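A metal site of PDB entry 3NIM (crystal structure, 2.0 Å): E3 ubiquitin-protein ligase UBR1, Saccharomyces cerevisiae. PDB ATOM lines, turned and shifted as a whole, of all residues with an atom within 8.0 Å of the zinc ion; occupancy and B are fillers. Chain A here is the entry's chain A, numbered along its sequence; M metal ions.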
ATOM      1  N   ARG A  23      30.320  13.654  27.472  1.00  0.00           N
ATOM      2  CA  ARG A  23      29.120  12.825  27.411  1.00  0.00           C
ATOM      3  C   ARG A  23      28.077  13.231  28.470  1.00  0.00           C
ATOM      4  O   ARG A  23      28.413  13.753  29.543  1.00  0.00           O
ATOM      5  CB  ARG A  23      29.457  11.342  27.504  1.00  0.00           C
ATOM      6  CG  ARG A  23      30.100  10.919  28.818  1.00  0.00           C
ATOM      7  CD  ARG A  23      30.633   9.510  28.731  1.00  0.00           C
ATOM      8  NE  ARG A  23      30.981   8.955  30.046  1.00  0.00           N
ATOM      9  CZ  ARG A  23      32.175   9.081  30.607  1.00  0.00           C
ATOM     10  NH1 ARG A  23      33.144   9.766  29.993  1.00  0.00           N
ATOM     11  NH2 ARG A  23      32.410   8.535  31.797  1.00  0.00           N
ATOM     12  N   CYS A  24      26.809  13.005  28.144  1.00  0.00           N
ATOM     13  CA  CYS A  24      25.691  13.327  29.017  1.00  0.00           C
ATOM     14  C   CYS A  24      24.836  12.082  29.173  1.00  0.00           C
ATOM     15  O   CYS A  24      24.301  11.567  28.177  1.00  0.00           O
ATOM     16  CB  CYS A  24      24.845  14.459  28.422  1.00  0.00           C
ATOM     17  SG  CYS A  24      23.399  14.824  29.445  1.00  0.00           S
ATOM     18  N   HIS A  25      24.701  11.612  30.404  1.00  0.00           N
ATOM     19  CA  HIS A  25      23.839  10.454  30.663  1.00  0.00           C
ATOM     20  C   HIS A  25      22.402  10.624  30.146  1.00  0.00           C
ATOM     21  O   HIS A  25      21.813   9.689  29.584  1.00  0.00           O
ATOM     22  CB  HIS A  25      23.810  10.100  32.151  1.00  0.00           C
ATOM     23  CG  HIS A  25      23.013   8.878  32.443  1.00  0.00           C
ATOM     24  ND1 HIS A  25      23.414   7.621  32.038  1.00  0.00           N
ATOM     25  CD2 HIS A  25      21.821   8.707  33.068  1.00  0.00           C
ATOM     26  CE1 HIS A  25      22.523   6.722  32.407  1.00  0.00           C
ATOM     27  NE2 HIS A  25      21.542   7.351  33.037  1.00  0.00           N
ATOM     28  N   GLU A  26      21.861  11.832  30.302  1.00  0.00           N
ATOM     29  CA  GLU A  26      20.489  12.091  29.897  1.00  0.00           C
ATOM     30  C   GLU A  26      20.349  12.278  28.386  1.00  0.00           C
ATOM     31  O   GLU A  26      19.391  11.812  27.815  1.00  0.00           O
ATOM     32  CB  GLU A  26      19.915  13.324  30.622  1.00  0.00           C
ATOM     33  CG  GLU A  26      19.597  13.123  32.086  1.00  0.00           C
ATOM     34  CD  GLU A  26      20.838  13.101  32.974  1.00  0.00           C
ATOM     35  OE1 GLU A  26      21.933  13.433  32.487  1.00  0.00           O
ATOM     36  OE2 GLU A  26      20.717  12.722  34.161  1.00  0.00           O
ATOM     37  N   CYS A  27      21.271  13.010  27.766  1.00  0.00           N
ATOM     38  CA  CYS A  27      21.108  13.326  26.349  1.00  0.00           C
ATOM     39  C   CYS A  27      21.626  12.232  25.427  1.00  0.00           C
ATOM     40  O   CYS A  27      21.111  12.055  24.335  1.00  0.00           O
ATOM     41  CB  CYS A  27      21.759  14.661  26.000  1.00  0.00           C
ATOM     42  SG  CYS A  27      20.992  15.998  26.909  1.00  0.00           S
ATOM     43  N   GLY A  28      22.660  11.525  25.871  1.00  0.00           N
ATOM     44  CA  GLY A  28      23.326  10.556  25.001  1.00  0.00           C
ATOM     45  C   GLY A  28      22.440   9.369  24.721  1.00  0.00           C
ATOM     46  O   GLY A  28      21.763   8.875  25.632  1.00  0.00           O
ATOM     47  N   LEU A  35      30.553  15.063  22.597  1.00  0.00           N
ATOM     48  CA  LEU A  35      30.571  16.416  22.002  1.00  0.00           C
ATOM     49  C   LEU A  35      31.919  17.074  22.230  1.00  0.00           C
ATOM     50  O   LEU A  35      32.612  16.784  23.214  1.00  0.00           O
ATOM     51  CB  LEU A  35      29.465  17.297  22.611  1.00  0.00           C
ATOM     52  CG  LEU A  35      27.993  16.879  22.443  1.00  0.00           C
ATOM     53  CD1 LEU A  35      27.050  17.502  23.473  1.00  0.00           C
ATOM     54  CD2 LEU A  35      27.493  17.150  21.012  1.00  0.00           C
ATOM     55  N   PHE A  40      29.567  21.579  22.785  1.00  0.00           N
ATOM     56  CA  PHE A  40      28.962  21.344  24.095  1.00  0.00           C
ATOM     57  C   PHE A  40      28.426  22.654  24.640  1.00  0.00           C
ATOM     58  O   PHE A  40      29.180  23.599  24.822  1.00  0.00           O
ATOM     59  CB  PHE A  40      30.008  20.764  25.046  1.00  0.00           C
ATOM     60  CG  PHE A  40      29.484  20.501  26.421  1.00  0.00           C
ATOM     61  CD1 PHE A  40      28.798  19.322  26.706  1.00  0.00           C
ATOM     62  CD2 PHE A  40      29.674  21.446  27.434  1.00  0.00           C
ATOM     63  CE1 PHE A  40      28.298  19.083  27.975  1.00  0.00           C
ATOM     64  CE2 PHE A  40      29.173  21.230  28.711  1.00  0.00           C
ATOM     65  CZ  PHE A  40      28.496  20.049  28.992  1.00  0.00           C
ATOM     66  N   ASN A  41      27.119  22.691  24.883  1.00  0.00           N
ATOM     67  CA  ASN A  41      26.455  23.869  25.447  1.00  0.00           C
ATOM     68  C   ASN A  41      26.062  23.582  26.895  1.00  0.00           C
ATOM     69  O   ASN A  41      25.077  22.854  27.138  1.00  0.00           O
ATOM     70  CB  ASN A  41      25.212  24.192  24.603  1.00  0.00           C
ATOM     71  CG  ASN A  41      24.537  25.517  24.991  1.00  0.00           C
ATOM     72  OD1 ASN A  41      24.600  25.952  26.138  1.00  0.00           O
ATOM     73  ND2 ASN A  41      23.884  26.148  24.024  1.00  0.00           N
ATOM     74  N   PRO A  42      26.793  24.164  27.859  1.00  0.00           N
ATOM     75  CA  PRO A  42      26.481  23.908  29.272  1.00  0.00           C
ATOM     76  C   PRO A  42      24.997  24.107  29.603  1.00  0.00           C
ATOM     77  O   PRO A  42      24.462  23.363  30.424  1.00  0.00           O
ATOM     78  CB  PRO A  42      27.355  24.933  30.003  1.00  0.00           C
ATOM     79  CG  PRO A  42      28.529  25.112  29.091  1.00  0.00           C
ATOM     80  CD  PRO A  42      27.920  25.113  27.724  1.00  0.00           C
ATOM     81  N   LYS A  43      24.327  25.040  28.938  1.00  0.00           N
ATOM     82  CA  LYS A  43      22.884  25.258  29.154  1.00  0.00           C
ATOM     83  C   LYS A  43      21.997  24.028  28.870  1.00  0.00           C
ATOM     84  O   LYS A  43      20.968  23.843  29.538  1.00  0.00           O
ATOM     85  CB  LYS A  43      22.393  26.506  28.404  1.00  0.00           C
ATOM     86  CG  LYS A  43      22.998  27.798  28.948  1.00  0.00           C
ATOM     87  CD  LYS A  43      22.539  29.046  28.171  1.00  0.00           C
ATOM     88  CE  LYS A  43      23.517  29.428  27.067  1.00  0.00           C
ATOM     89  NZ  LYS A  43      23.095  30.649  26.286  1.00  0.00           N
ATOM     90  N   ASP A  44      22.392  23.202  27.901  1.00  0.00           N
ATOM     91  CA  ASP A  44      21.603  21.989  27.576  1.00  0.00           C
ATOM     92  C   ASP A  44      21.628  20.948  28.690  1.00  0.00           C
ATOM     93  O   ASP A  44      20.788  20.034  28.718  1.00  0.00           O
ATOM     94  CB  ASP A  44      22.120  21.320  26.293  1.00  0.00           C
ATOM     95  CG  ASP A  44      21.802  22.120  25.027  1.00  0.00           C
ATOM     96  OD1 ASP A  44      20.767  22.825  24.970  1.00  0.00           O
ATOM     97  OD2 ASP A  44      22.596  22.014  24.070  1.00  0.00           O
ATOM     98  N   HIS A  45      22.572  21.096  29.624  1.00  0.00           N
ATOM     99  CA  HIS A  45      22.901  20.006  30.545  1.00  0.00           C
ATOM    100  C   HIS A  45      23.054  20.429  32.011  1.00  0.00           C
ATOM    101  O   HIS A  45      23.814  19.815  32.761  1.00  0.00           O
ATOM    102  CB  HIS A  45      24.174  19.292  30.051  1.00  0.00           C
ATOM    103  CG  HIS A  45      24.212  19.064  28.570  1.00  0.00           C
ATOM    104  ND1 HIS A  45      23.397  18.145  27.928  1.00  0.00           N
ATOM    105  CD2 HIS A  45      24.954  19.648  27.600  1.00  0.00           C
ATOM    106  CE1 HIS A  45      23.666  18.164  26.631  1.00  0.00           C
ATOM    107  NE2 HIS A  45      24.604  19.069  26.407  1.00  0.00           N
ATOM    108  N   VAL A  46      22.318  21.464  32.406  1.00  0.00           N
ATOM    109  CA  VAL A  46      22.340  21.962  33.792  1.00  0.00           C
ATOM    110  C   VAL A  46      21.916  20.909  34.831  1.00  0.00           C
ATOM    111  O   VAL A  46      22.644  20.665  35.812  1.00  0.00           O
ATOM    112  CB  VAL A  46      21.470  23.221  33.994  1.00  0.00           C
ATOM    113  CG1 VAL A  46      21.743  23.828  35.347  1.00  0.00           C
ATOM    114  CG2 VAL A  46      21.711  24.255  32.893  1.00  0.00           C
ATOM    115  N   ASN A  47      20.759  20.289  34.623  1.00  0.00           N
ATOM    116  CA  ASN A  47      20.288  19.258  35.547  1.00  0.00           C
ATOM    117  C   ASN A  47      20.665  17.842  35.111  1.00  0.00           C
ATOM    118  O   ASN A  47      19.973  16.871  35.435  1.00  0.00           O
ATOM    119  CB  ASN A  47      18.786  19.391  35.806  1.00  0.00           C
ATOM    120  CG  ASN A  47      18.466  20.566  36.716  1.00  0.00           C
ATOM    121  OD1 ASN A  47      18.583  21.732  36.316  1.00  0.00           O
ATOM    122  ND2 ASN A  47      18.094  20.273  37.973  1.00  0.00           N
ATOM    123  N   HIS A  48      21.764  17.749  34.359  1.00  0.00           N
ATOM    124  CA  HIS A  48      22.182  16.485  33.754  1.00  0.00           C
ATOM    125  C   HIS A  48      23.505  15.984  34.335  1.00  0.00           C
ATOM    126  O   HIS A  48      24.232  16.762  34.941  1.00  0.00           O
ATOM    127  CB  HIS A  48      22.275  16.656  32.239  1.00  0.00           C
ATOM    128  CG  HIS A  48      20.946  16.890  31.578  1.00  0.00           C
ATOM    129  ND1 HIS A  48      20.797  16.881  30.204  1.00  0.00           N
ATOM    130  CD2 HIS A  48      19.716  17.124  32.091  1.00  0.00           C
ATOM    131  CE1 HIS A  48      19.528  17.119  29.908  1.00  0.00           C
ATOM    132  NE2 HIS A  48      18.859  17.276  31.031  1.00  0.00           N
ATOM    133  N   HIS A  49      23.785  14.690  34.178  1.00  0.00           N
ATOM    134  CA  HIS A  49      25.023  14.085  34.660  1.00  0.00           C
ATOM    135  C   HIS A  49      26.056  13.977  33.537  1.00  0.00           C
ATOM    136  O   HIS A  49      26.023  13.027  32.739  1.00  0.00           O
ATOM    137  CB  HIS A  49      24.754  12.677  35.211  1.00  0.00           C
ATOM    138  CG  HIS A  49      23.850  12.659  36.413  1.00  0.00           C
ATOM    139  ND1 HIS A  49      22.515  12.980  36.342  1.00  0.00           N
ATOM    140  CD2 HIS A  49      24.089  12.310  37.695  1.00  0.00           C
ATOM    141  CE1 HIS A  49      21.971  12.857  37.547  1.00  0.00           C
ATOM    142  NE2 HIS A  49      22.912  12.442  38.379  1.00  0.00           N
ATOM    143  N   VAL A  50      26.976  14.941  33.506  1.00  0.00           N
ATOM    144  CA  VAL A  50      27.993  15.080  32.453  1.00  0.00           C
ATOM    145  C   VAL A  50      29.349  14.567  32.917  1.00  0.00           C
ATOM    146  O   VAL A  50      29.728  14.778  34.063  1.00  0.00           O
ATOM    147  CB  VAL A  50      28.147  16.556  32.030  1.00  0.00           C
ATOM    148  CG1 VAL A  50      29.340  16.758  31.049  1.00  0.00           C
ATOM    149  CG2 VAL A  50      26.858  17.066  31.419  1.00  0.00           C
ATOM    150  N   TRP A  71      21.436  11.485  19.982  1.00  0.00           N
ATOM    151  CA  TRP A  71      20.871  12.287  21.087  1.00  0.00           C
ATOM    152  C   TRP A  71      19.375  12.110  21.313  1.00  0.00           C
ATOM    153  O   TRP A  71      18.606  12.014  20.360  1.00  0.00           O
ATOM    154  CB  TRP A  71      21.158  13.780  20.866  1.00  0.00           C
ATOM    155  CG  TRP A  71      22.579  13.990  20.559  1.00  0.00           C
ATOM    156  CD1 TRP A  71      23.117  14.311  19.350  1.00  0.00           C
ATOM    157  CD2 TRP A  71      23.667  13.853  21.476  1.00  0.00           C
ATOM    158  NE1 TRP A  71      24.489  14.376  19.455  1.00  0.00           N
ATOM    159  CE2 TRP A  71      24.859  14.091  20.739  1.00  0.00           C
ATOM    160  CE3 TRP A  71      23.767  13.523  22.838  1.00  0.00           C
ATOM    161  CZ2 TRP A  71      26.134  14.036  21.331  1.00  0.00           C
ATOM    162  CZ3 TRP A  71      25.036  13.457  23.424  1.00  0.00           C
ATOM    163  CH2 TRP A  71      26.206  13.726  22.670  1.00  0.00           C
ATOM    164  N   SER A  73      17.540  14.339  23.172  1.00  0.00           N
ATOM    165  CA  SER A  73      16.961  15.692  23.121  1.00  0.00           C
ATOM    166  C   SER A  73      17.609  16.541  22.022  1.00  0.00           C
ATOM    167  O   SER A  73      18.739  16.291  21.642  1.00  0.00           O
ATOM    168  CB  SER A  73      17.139  16.417  24.470  1.00  0.00           C
ATOM    169  OG  SER A  73      16.724  15.618  25.578  1.00  0.00           O
ATOM    170  N   PRO A  74      16.868  17.540  21.507  1.00  0.00           N
ATOM    171  CA  PRO A  74      17.463  18.597  20.686  1.00  0.00           C
ATOM    172  C   PRO A  74      18.621  19.250  21.432  1.00  0.00           C
ATOM    173  O   PRO A  74      18.455  19.642  22.601  1.00  0.00           O
ATOM    174  CB  PRO A  74      16.313  19.611  20.549  1.00  0.00           C
ATOM    175  CG  PRO A  74      15.297  19.214  21.606  1.00  0.00           C
ATOM    176  CD  PRO A  74      15.416  17.740  21.640  1.00  0.00           C
ATOM    177  N   LEU A  75      19.791  19.326  20.788  1.00  0.00           N
ATOM    178  CA  LEU A  75      20.937  20.101  21.294  1.00  0.00           C
ATOM    179  C   LEU A  75      21.008  21.467  20.613  1.00  0.00           C
ATOM    180  O   LEU A  75      20.630  21.627  19.455  1.00  0.00           O
ATOM    181  CB  LEU A  75      22.270  19.381  21.077  1.00  0.00           C
ATOM    182  CG  LEU A  75      22.551  18.002  21.670  1.00  0.00           C
ATOM    183  CD1 LEU A  75      23.933  17.551  21.261  1.00  0.00           C
ATOM    184  CD2 LEU A  75      22.399  17.982  23.169  1.00  0.00           C
HETATM  185 ZN    ZN M   1      22.331  16.508  28.673  1.00  0.00          ZN
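The side-chain sulfur (SG) of Cys 24 sits close to the backbone NH (N) of Glu 26 (3.5 Å). ND1 of His 48 sits close to O of Asp 44 (3.5 Å).
The zinc ion is bound by a ring nitrogen (ND1) of His 45 (2.1 Å). The zinc ion is bound by SG of Cys 24 (2.1 Å). The zinc ion is bound by ND1 of His 48 (2.2 Å). SG of Cys 27 is bound to the zinc ion, 2.3 Å away.
O of Asp 44 touches the zinc ion, at 3.8 Å. Five residues have an atom within 4 Å of the zinc ion: Cys 24, Cys 27, Asp 44, His 45 and His 48. Along chain A the residues within 4 Å of the zinc ion span positions 24 to 48. The nearest printed residue that does not touch the zinc ion is Glu 26 (4.4 Å).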
